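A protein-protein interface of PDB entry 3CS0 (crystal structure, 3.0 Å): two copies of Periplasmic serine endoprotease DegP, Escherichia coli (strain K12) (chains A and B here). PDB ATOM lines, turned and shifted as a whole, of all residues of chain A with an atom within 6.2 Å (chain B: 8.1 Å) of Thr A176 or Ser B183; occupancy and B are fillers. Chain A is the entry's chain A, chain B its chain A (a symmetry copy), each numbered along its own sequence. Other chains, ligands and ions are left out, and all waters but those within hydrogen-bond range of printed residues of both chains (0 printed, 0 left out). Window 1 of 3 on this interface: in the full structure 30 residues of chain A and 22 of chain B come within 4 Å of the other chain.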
ATOM      1  N   MET A  23       5.834  17.499   2.309  1.00  0.00           N
ATOM      2  CA  MET A  23       6.811  17.610   3.398  1.00  0.00           C
ATOM      3  C   MET A  23       8.176  16.979   3.176  1.00  0.00           C
ATOM      4  O   MET A  23       9.182  17.538   3.594  1.00  0.00           O
ATOM      5  CB  MET A  23       6.205  17.142   4.722  1.00  0.00           C
ATOM      6  CG  MET A  23       5.149  18.110   5.222  1.00  0.00           C
ATOM      7  SD  MET A  23       4.312  17.653   6.895  1.00  0.00           S
ATOM      8  CE  MET A  23       3.228  16.140   6.317  1.00  0.00           C
ATOM      9  N   ALA A 166       3.435  27.529   5.622  1.00  0.00           N
ATOM     10  CA  ALA A 166       4.900  27.640   5.710  1.00  0.00           C
ATOM     11  C   ALA A 166       5.402  26.394   6.395  1.00  0.00           C
ATOM     12  O   ALA A 166       4.797  25.950   7.380  1.00  0.00           O
ATOM     13  CB  ALA A 166       5.299  28.855   6.519  1.00  0.00           C
ATOM     14  N   ILE A 167       6.498  25.833   5.876  1.00  0.00           N
ATOM     15  CA  ILE A 167       7.102  24.609   6.419  1.00  0.00           C
ATOM     16  C   ILE A 167       8.579  24.853   6.711  1.00  0.00           C
ATOM     17  O   ILE A 167       9.296  25.387   5.857  1.00  0.00           O
ATOM     18  CB  ILE A 167       7.006  23.490   5.399  1.00  0.00           C
ATOM     19  CG1 ILE A 167       5.561  23.357   4.927  1.00  0.00           C
ATOM     20  CG2 ILE A 167       7.519  22.201   5.996  1.00  0.00           C
ATOM     21  CD1 ILE A 167       5.433  22.704   3.576  1.00  0.00           C
ATOM     22  N   GLY A 168       9.039  24.459   7.896  1.00  0.00           N
ATOM     23  CA  GLY A 168      10.437  24.674   8.240  1.00  0.00           C
ATOM     24  C   GLY A 168      10.784  24.190   9.635  1.00  0.00           C
ATOM     25  O   GLY A 168       9.976  23.520  10.273  1.00  0.00           O
ATOM     26  N   ASN A 169      11.968  24.544  10.129  1.00  0.00           N
ATOM     27  CA  ASN A 169      12.393  24.096  11.443  1.00  0.00           C
ATOM     28  C   ASN A 169      12.567  25.160  12.514  1.00  0.00           C
ATOM     29  O   ASN A 169      13.684  25.522  12.855  1.00  0.00           O
ATOM     30  CB  ASN A 169      13.694  23.322  11.322  1.00  0.00           C
ATOM     31  CG  ASN A 169      13.988  22.489  12.563  1.00  0.00           C
ATOM     32  OD1 ASN A 169      14.663  21.450  12.492  1.00  0.00           O
ATOM     33  ND2 ASN A 169      13.476  22.934  13.706  1.00  0.00           N
ATOM     34  N   PRO A 170      11.460  25.658  13.086  1.00  0.00           N
ATOM     35  CA  PRO A 170      11.594  26.681  14.130  1.00  0.00           C
ATOM     36  C   PRO A 170      12.322  26.121  15.359  1.00  0.00           C
ATOM     37  O   PRO A 170      11.974  25.053  15.859  1.00  0.00           O
ATOM     38  CB  PRO A 170      10.140  27.054  14.432  1.00  0.00           C
ATOM     39  CG  PRO A 170       9.387  25.770  14.168  1.00  0.00           C
ATOM     40  CD  PRO A 170      10.046  25.283  12.884  1.00  0.00           C
ATOM     41  N   LEU A 173      13.063  22.297  16.649  1.00  0.00           N
ATOM     42  CA  LEU A 173      12.054  21.331  17.089  1.00  0.00           C
ATOM     43  C   LEU A 173      11.783  20.225  16.055  1.00  0.00           C
ATOM     44  O   LEU A 173      11.362  19.114  16.427  1.00  0.00           O
ATOM     45  CB  LEU A 173      10.724  22.047  17.369  1.00  0.00           C
ATOM     46  CG  LEU A 173      10.578  22.844  18.655  1.00  0.00           C
ATOM     47  CD1 LEU A 173       9.451  23.856  18.525  1.00  0.00           C
ATOM     48  CD2 LEU A 173      10.323  21.873  19.780  1.00  0.00           C
ATOM     49  N   GLY A 174      11.999  20.535  14.772  1.00  0.00           N
ATOM     50  CA  GLY A 174      11.724  19.568  13.719  1.00  0.00           C
ATOM     51  C   GLY A 174      10.825  20.156  12.641  1.00  0.00           C
ATOM     52  O   GLY A 174      10.552  21.359  12.696  1.00  0.00           O
ATOM     53  N   GLU A 175      10.359  19.348  11.680  1.00  0.00           N
ATOM     54  CA  GLU A 175       9.508  19.865  10.601  1.00  0.00           C
ATOM     55  C   GLU A 175       8.205  20.392  11.141  1.00  0.00           C
ATOM     56  O   GLU A 175       7.340  19.644  11.592  1.00  0.00           O
ATOM     57  CB  GLU A 175       9.196  18.809   9.545  1.00  0.00           C
ATOM     58  CG  GLU A 175       9.681  19.245   8.167  1.00  0.00           C
ATOM     59  CD  GLU A 175       8.945  18.598   6.992  1.00  0.00           C
ATOM     60  OE1 GLU A 175       9.340  18.896   5.839  1.00  0.00           O
ATOM     61  OE2 GLU A 175       7.985  17.814   7.209  1.00  0.00           O
ATOM     62  N   THR A 176       8.055  21.699  11.086  1.00  0.00           N
ATOM     63  CA  THR A 176       6.855  22.307  11.596  1.00  0.00           C
ATOM     64  C   THR A 176       6.085  22.985  10.473  1.00  0.00           C
ATOM     65  O   THR A 176       6.688  23.661   9.610  1.00  0.00           O
ATOM     66  CB  THR A 176       7.231  23.312  12.692  1.00  0.00           C
ATOM     67  OG1 THR A 176       7.637  22.585  13.853  1.00  0.00           O
ATOM     68  CG2 THR A 176       6.079  24.248  13.018  1.00  0.00           C
ATOM     69  N   VAL A 177       4.768  22.775  10.446  1.00  0.00           N
ATOM     70  CA  VAL A 177       3.964  23.440   9.434  1.00  0.00           C
ATOM     71  C   VAL A 177       2.949  24.342  10.108  1.00  0.00           C
ATOM     72  O   VAL A 177       2.261  23.946  11.049  1.00  0.00           O
ATOM     73  CB  VAL A 177       3.279  22.437   8.432  1.00  0.00           C
ATOM     74  CG1 VAL A 177       3.505  21.006   8.864  1.00  0.00           C
ATOM     75  CG2 VAL A 177       1.811  22.740   8.291  1.00  0.00           C
ATOM     76  N   THR A 178       2.900  25.578   9.629  1.00  0.00           N
ATOM     77  CA  THR A 178       1.994  26.601  10.141  1.00  0.00           C
ATOM     78  C   THR A 178       1.347  27.289   8.927  1.00  0.00           C
ATOM     79  O   THR A 178       1.930  27.288   7.827  1.00  0.00           O
ATOM     80  CB  THR A 178       2.783  27.622  11.016  1.00  0.00           C
ATOM     81  OG1 THR A 178       3.767  28.314  10.227  1.00  0.00           O
ATOM     82  CG2 THR A 178       3.490  26.880  12.148  1.00  0.00           C
ATOM     83  N   ASN A 209      13.128  28.807  10.763  1.00  0.00           N
ATOM     84  CA  ASN A 209      12.340  28.774   9.542  1.00  0.00           C
ATOM     85  C   ASN A 209      13.053  29.261   8.270  1.00  0.00           C
ATOM     86  O   ASN A 209      12.665  28.887   7.167  1.00  0.00           O
ATOM     87  CB  ASN A 209      11.055  29.588   9.741  1.00  0.00           C
ATOM     88  CG  ASN A 209       9.965  28.786  10.397  1.00  0.00           C
ATOM     89  OD1 ASN A 209       9.642  27.694   9.940  1.00  0.00           O
ATOM     90  ND2 ASN A 209       9.384  29.319  11.468  1.00  0.00           N
ATOM     91  N   ARG B 159      -3.672  13.958  11.838  1.00  0.00           N
ATOM     92  CA  ARG B 159      -2.611  14.080  10.851  1.00  0.00           C
ATOM     93  C   ARG B 159      -2.149  15.521  10.870  1.00  0.00           C
ATOM     94  O   ARG B 159      -2.928  16.427  11.162  1.00  0.00           O
ATOM     95  CB  ARG B 159      -3.116  13.701   9.469  1.00  0.00           C
ATOM     96  CG  ARG B 159      -3.076  12.216   9.198  1.00  0.00           C
ATOM     97  CD  ARG B 159      -3.435  11.966   7.754  1.00  0.00           C
ATOM     98  NE  ARG B 159      -4.760  12.499   7.472  1.00  0.00           N
ATOM     99  CZ  ARG B 159      -5.221  12.737   6.253  1.00  0.00           C
ATOM    100  NH1 ARG B 159      -4.446  12.483   5.200  1.00  0.00           N
ATOM    101  NH2 ARG B 159      -6.448  13.232   6.096  1.00  0.00           N
ATOM    102  N   VAL B 160      -0.884  15.750  10.556  1.00  0.00           N
ATOM    103  CA  VAL B 160      -0.391  17.099  10.606  1.00  0.00           C
ATOM    104  C   VAL B 160      -1.197  18.150   9.873  1.00  0.00           C
ATOM    105  O   VAL B 160      -1.442  19.227  10.429  1.00  0.00           O
ATOM    106  CB  VAL B 160       1.074  17.157  10.222  1.00  0.00           C
ATOM    107  CG1 VAL B 160       1.402  18.439   9.479  1.00  0.00           C
ATOM    108  CG2 VAL B 160       1.868  17.147  11.489  1.00  0.00           C
ATOM    109  N   GLY B 161      -1.651  17.896   8.657  1.00  0.00           N
ATOM    110  CA  GLY B 161      -2.429  18.974   8.036  1.00  0.00           C
ATOM    111  C   GLY B 161      -3.773  19.415   8.670  1.00  0.00           C
ATOM    112  O   GLY B 161      -4.342  20.438   8.279  1.00  0.00           O
ATOM    113  N   ASP B 162      -4.270  18.650   9.650  1.00  0.00           N
ATOM    114  CA  ASP B 162      -5.563  18.893  10.292  1.00  0.00           C
ATOM    115  C   ASP B 162      -5.839  20.222  10.970  1.00  0.00           C
ATOM    116  O   ASP B 162      -4.952  20.830  11.561  1.00  0.00           O
ATOM    117  CB  ASP B 162      -5.850  17.762  11.266  1.00  0.00           C
ATOM    118  CG  ASP B 162      -6.083  16.439  10.549  1.00  0.00           C
ATOM    119  OD1 ASP B 162      -6.085  16.459   9.292  1.00  0.00           O
ATOM    120  OD2 ASP B 162      -6.264  15.390  11.224  1.00  0.00           O
ATOM    121  N   THR B 164      -7.553  22.800  13.782  1.00  0.00           N
ATOM    122  CA  THR B 164      -7.792  22.726  15.220  1.00  0.00           C
ATOM    123  C   THR B 164      -8.290  24.042  15.795  1.00  0.00           C
ATOM    124  O   THR B 164      -7.880  25.113  15.348  1.00  0.00           O
ATOM    125  CB  THR B 164      -6.501  22.454  15.974  1.00  0.00           C
ATOM    126  OG1 THR B 164      -5.582  23.529  15.712  1.00  0.00           O
ATOM    127  CG2 THR B 164      -5.879  21.149  15.546  1.00  0.00           C
ATOM    128  N   GLY B 180      -6.220  27.217  14.411  1.00  0.00           N
ATOM    129  CA  GLY B 180      -4.997  26.994  13.662  1.00  0.00           C
ATOM    130  C   GLY B 180      -4.944  25.593  13.082  1.00  0.00           C
ATOM    131  O   GLY B 180      -5.979  25.029  12.692  1.00  0.00           O
ATOM    132  N   ILE B 181      -3.743  25.024  12.997  1.00  0.00           N
ATOM    133  CA  ILE B 181      -3.605  23.662  12.484  1.00  0.00           C
ATOM    134  C   ILE B 181      -2.653  22.834  13.321  1.00  0.00           C
ATOM    135  O   ILE B 181      -1.927  23.365  14.165  1.00  0.00           O
ATOM    136  CB  ILE B 181      -3.090  23.628  11.026  1.00  0.00           C
ATOM    137  CG1 ILE B 181      -1.668  24.186  10.943  1.00  0.00           C
ATOM    138  CG2 ILE B 181      -4.039  24.399  10.122  1.00  0.00           C
ATOM    139  CD1 ILE B 181      -1.100  24.172   9.510  1.00  0.00           C
ATOM    140  N   VAL B 182      -2.692  21.524  13.110  1.00  0.00           N
ATOM    141  CA  VAL B 182      -1.793  20.604  13.785  1.00  0.00           C
ATOM    142  C   VAL B 182      -0.443  20.867  13.109  1.00  0.00           C
ATOM    143  O   VAL B 182      -0.276  20.620  11.920  1.00  0.00           O
ATOM    144  CB  VAL B 182      -2.212  19.154  13.519  1.00  0.00           C
ATOM    145  CG1 VAL B 182      -1.034  18.219  13.764  1.00  0.00           C
ATOM    146  CG2 VAL B 182      -3.412  18.784  14.406  1.00  0.00           C
ATOM    147  N   SER B 183       0.524  21.390  13.838  1.00  0.00           N
ATOM    148  CA  SER B 183       1.794  21.662  13.199  1.00  0.00           C
ATOM    149  C   SER B 183       2.717  20.455  13.230  1.00  0.00           C
ATOM    150  O   SER B 183       3.583  20.307  12.363  1.00  0.00           O
ATOM    151  CB  SER B 183       2.493  22.833  13.886  1.00  0.00           C
ATOM    152  OG  SER B 183       1.700  24.002  13.854  1.00  0.00           O
ATOM    153  N   ALA B 184       2.527  19.583  14.210  1.00  0.00           N
ATOM    154  CA  ALA B 184       3.402  18.431  14.338  1.00  0.00           C
ATOM    155  C   ALA B 184       2.839  17.429  15.347  1.00  0.00           C
ATOM    156  O   ALA B 184       1.991  17.783  16.191  1.00  0.00           O
ATOM    157  CB  ALA B 184       4.785  18.906  14.796  1.00  0.00           C
ATOM    158  N   LEU B 185       3.310  16.184  15.272  1.00  0.00           N
ATOM    159  CA  LEU B 185       2.846  15.176  16.208  1.00  0.00           C
ATOM    160  C   LEU B 185       4.038  14.553  16.922  1.00  0.00           C
ATOM    161  O   LEU B 185       5.144  14.544  16.401  1.00  0.00           O
ATOM    162  CB  LEU B 185       2.040  14.119  15.473  1.00  0.00           C
ATOM    163  CG  LEU B 185       0.781  14.684  14.812  1.00  0.00           C
ATOM    164  CD1 LEU B 185       0.058  13.627  14.029  1.00  0.00           C
ATOM    165  CD2 LEU B 185      -0.143  15.223  15.873  1.00  0.00           C
ATOM    166  N   ARG B 187       5.743  15.635  19.603  1.00  0.00           N
ATOM    167  CA  ARG B 187       6.803  16.463  20.183  1.00  0.00           C
ATOM    168  C   ARG B 187       6.998  16.102  21.641  1.00  0.00           C
ATOM    169  O   ARG B 187       6.035  15.857  22.364  1.00  0.00           O
ATOM    170  CB  ARG B 187       6.492  17.960  20.062  1.00  0.00           C
ATOM    171  CG  ARG B 187       6.446  18.491  18.634  1.00  0.00           C
ATOM    172  CD  ARG B 187       7.744  18.260  17.855  1.00  0.00           C
ATOM    173  NE  ARG B 187       7.852  19.178  16.725  1.00  0.00           N
ATOM    174  CZ  ARG B 187       8.195  18.798  15.502  1.00  0.00           C
ATOM    175  NH1 ARG B 187       8.466  17.526  15.266  1.00  0.00           N
ATOM    176  NH2 ARG B 187       8.239  19.671  14.506  1.00  0.00           N
ATOM    177  N   PHE B 198       3.311  15.270  22.811  1.00  0.00           N
ATOM    178  CA  PHE B 198       2.539  16.454  22.452  1.00  0.00           C
ATOM    179  C   PHE B 198       2.120  16.677  21.021  1.00  0.00           C
ATOM    180  O   PHE B 198       2.873  16.422  20.091  1.00  0.00           O
ATOM    181  CB  PHE B 198       3.284  17.722  22.845  1.00  0.00           C
ATOM    182  CG  PHE B 198       3.479  17.888  24.301  1.00  0.00           C
ATOM    183  CD1 PHE B 198       2.413  17.768  25.173  1.00  0.00           C
ATOM    184  CD2 PHE B 198       4.728  18.215  24.805  1.00  0.00           C
ATOM    185  CE1 PHE B 198       2.588  17.975  26.540  1.00  0.00           C
ATOM    186  CE2 PHE B 198       4.917  18.424  26.164  1.00  0.00           C
ATOM    187  CZ  PHE B 198       3.850  18.305  27.035  1.00  0.00           C
ATOM    188  N   ILE B 199       0.907  17.190  20.866  1.00  0.00           N
ATOM    189  CA  ILE B 199       0.394  17.591  19.572  1.00  0.00           C
ATOM    190  C   ILE B 199       0.848  19.053  19.550  1.00  0.00           C
ATOM    191  O   ILE B 199       0.723  19.763  20.569  1.00  0.00           O
ATOM    192  CB  ILE B 199      -1.120  17.600  19.548  1.00  0.00           C
ATOM    193  CG1 ILE B 199      -1.626  16.184  19.630  1.00  0.00           C
ATOM    194  CG2 ILE B 199      -1.638  18.340  18.303  1.00  0.00           C
ATOM    195  CD1 ILE B 199      -3.099  16.143  19.874  1.00  0.00           C
ATOM    196  N   GLN B 200       1.385  19.495  18.416  1.00  0.00           N
ATOM    197  CA  GLN B 200       1.854  20.872  18.287  1.00  0.00           C
ATOM    198  C   GLN B 200       0.887  21.684  17.426  1.00  0.00           C
ATOM    199  O   GLN B 200       0.484  21.229  16.346  1.00  0.00           O
ATOM    200  CB  GLN B 200       3.240  20.883  17.654  1.00  0.00           C
ATOM    201  CG  GLN B 200       4.028  22.129  17.979  1.00  0.00           C
ATOM    202  CD  GLN B 200       5.347  22.189  17.243  1.00  0.00           C
ATOM    203  OE1 GLN B 200       6.190  21.287  17.369  1.00  0.00           O
ATOM    204  NE2 GLN B 200       5.539  23.259  16.462  1.00  0.00           N
ATOM    205  N   THR B 201       0.507  22.878  17.880  1.00  0.00           N
ATOM    206  CA  THR B 201      -0.422  23.682  17.086  1.00  0.00           C
ATOM    207  C   THR B 201      -0.117  25.172  17.073  1.00  0.00           C
ATOM    208  O   THR B 201       0.460  25.707  18.026  1.00  0.00           O
ATOM    209  CB  THR B 201      -1.862  23.513  17.572  1.00  0.00           C
ATOM    210  OG1 THR B 201      -2.744  24.193  16.667  1.00  0.00           O
ATOM    211  CG2 THR B 201      -2.017  24.097  18.973  1.00  0.00           C
ATOM    212  N   ASP B 202      -0.506  25.849  15.995  1.00  0.00           N
ATOM    213  CA  ASP B 202      -0.261  27.284  15.920  1.00  0.00           C
ATOM    214  C   ASP B 202      -1.502  28.107  16.265  1.00  0.00           C
ATOM    215  O   ASP B 202      -1.526  29.308  16.007  1.00  0.00           O
ATOM    216  CB  ASP B 202       0.290  27.700  14.548  1.00  0.00           C
ATOM    217  CG  ASP B 202      -0.642  27.335  13.396  1.00  0.00           C
ATOM    218  OD1 ASP B 202      -1.721  26.750  13.665  1.00  0.00           O
ATOM    219  OD2 ASP B 202      -0.296  27.632  12.220  1.00  0.00           O
ATOM    220  N   ALA B 203      -2.539  27.468  16.825  1.00  0.00           N
ATOM    221  CA  ALA B 203      -3.722  28.219  17.259  1.00  0.00           C
ATOM    222  C   ALA B 203      -3.166  28.944  18.487  1.00  0.00           C
ATOM    223  O   ALA B 203      -2.423  28.337  19.265  1.00  0.00           O
ATOM    224  CB  ALA B 203      -4.847  27.293  17.663  1.00  0.00           C
ATOM    225  N   GLY B 237       3.197  31.202  18.011  1.00  0.00           N
ATOM    226  CA  GLY B 237       2.814  30.326  16.926  1.00  0.00           C
ATOM    227  C   GLY B 237       3.152  28.884  17.231  1.00  0.00           C
ATOM    228  O   GLY B 237       2.890  28.001  16.409  1.00  0.00           O
ATOM    229  N   ILE B 238       3.712  28.631  18.415  1.00  0.00           N
ATOM    230  CA  ILE B 238       4.086  27.275  18.794  1.00  0.00           C
ATOM    231  C   ILE B 238       3.480  26.831  20.136  1.00  0.00           C
ATOM    232  O   ILE B 238       3.971  27.209  21.197  1.00  0.00           O
ATOM    233  CB  ILE B 238       5.612  27.165  18.886  1.00  0.00           C
ATOM    234  CG1 ILE B 238       6.252  27.597  17.571  1.00  0.00           C
ATOM    235  CG2 ILE B 238       6.018  25.756  19.213  1.00  0.00           C
ATOM    236  CD1 ILE B 238       7.785  27.476  17.594  1.00  0.00           C
ATOM    237  N   GLY B 239       2.419  26.035  20.098  1.00  0.00           N
ATOM    238  CA  GLY B 239       1.809  25.568  21.336  1.00  0.00           C
ATOM    239  C   GLY B 239       1.707  24.052  21.383  1.00  0.00           C
ATOM    240  O   GLY B 239       1.679  23.390  20.334  1.00  0.00           O
ATOM    241  N   PHE B 240       1.637  23.490  22.586  1.00  0.00           N
ATOM    242  CA  PHE B 240       1.574  22.031  22.737  1.00  0.00           C
ATOM    243  C   PHE B 240       0.386  21.526  23.529  1.00  0.00           C
ATOM    244  O   PHE B 240      -0.061  22.183  24.476  1.00  0.00           O
ATOM    245  CB  PHE B 240       2.842  21.523  23.431  1.00  0.00           C
ATOM    246  CG  PHE B 240       4.104  21.952  22.762  1.00  0.00           C
ATOM    247  CD1 PHE B 240       4.787  23.068  23.203  1.00  0.00           C
ATOM    248  CD2 PHE B 240       4.570  21.278  21.642  1.00  0.00           C
ATOM    249  CE1 PHE B 240       5.914  23.509  22.534  1.00  0.00           C
ATOM    250  CE2 PHE B 240       5.694  21.713  20.963  1.00  0.00           C
ATOM    251  CZ  PHE B 240       6.367  22.829  21.410  1.00  0.00           C
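N of Ile B181 is in hydrogen-bond range of OD1 of Asp B202 (2.7 Å). The guanidinium group (NE) of Arg B187 sits at hydrogen-bond distance from the side-chain amide oxygen (OE1) of Gln B200 (2.8 Å). O of Ala B184 sits at hydrogen-bond distance from N of Gln B200 (2.9 Å). OE1 of Glu A175 sits close to O of Met A23 (2.6 Å). The backbone carbonyl oxygen (O) of Gly A168 sits at hydrogen-bond distance from the backbone NH (N) of Thr A176 (2.8 Å). The backbone carbonyl oxygen (O) of Ile B181 sits at hydrogen-bond distance from the side-chain hydroxyl (OG1) of Thr B201 (2.8 Å).
O of Val A177 lies within hydrogen-bond range of OG of Ser B183. NH2 of Arg B187 lies close to O of Gly A174, 3.4 Å away. The side-chain hydroxyl of Thr A176 sits at hydrogen-bond distance from the guanidinium group of Arg B187 (3.0 Å). The side-chain amide nitrogen (NE2) of Gln B200 is in hydrogen-bond range of the side-chain hydroxyl (OG1) of Thr A176 (3.4 Å). The backbone carbonyl oxygen (O) of Glu A175 lies within hydrogen-bond range of the guanidinium group (NH2) of Arg B187, at 3.0 Å.
No position is printed for both chains.
Of the 13 printed residues of chain A, 8 touch a printed residue of chain B. Printed residues of chain A that touch a printed residue of chain B: Met A23, Pro A170, Leu A173, Gly A174, Glu A175, Thr A176, Val A177 and Thr A178. Hydrophobic or aromatic side chains of chain B within 4 Å of the printed part of chain A: Val B160, Ile B181 and Ile B238. Along chain B the printed residues that touch a printed residue of chain A span positions 160 to 238. Among the printed residues, no Asp or Glu carboxylate lies within 4 Å of a Lys or Arg side-chain nitrogen of the other chain.
Among the printed residues, pairs that only touch across the chains: Thr A178 with Asp B202, Leu A173 with Arg B187, Val A177 with Val B160, Val A177 with Ile B181, Thr A178 with Ser B183, Glu A175 with Ser B183, Thr A176 with Ser B183, Pro A170 with Ile B238, Met A23 with Val B160, Leu A173 with Ile B238 and Thr A178 with Ile B181.
Thr A176 touches three residues of chain B. Ser B183 touches just these residues of chain A: Glu A175, Thr A176, Val A177 and Thr A178. Printed residues of chain A within 4 Å of Arg B187: Leu A173, Gly A174, Glu A175 and Thr A176. Of the printed residues of chain A, Ile B181 touches Val A177 and Thr A178. The nearest residue of chain B that does not touch Thr A176 is Ala B184 (4.7 Å). The nearest residue of chain A that does not touch Ser B183 is Met A23 (6.1 Å). The nearest printed residue of chain B that does not touch Met A23 is Gly B161 (5.7 Å).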
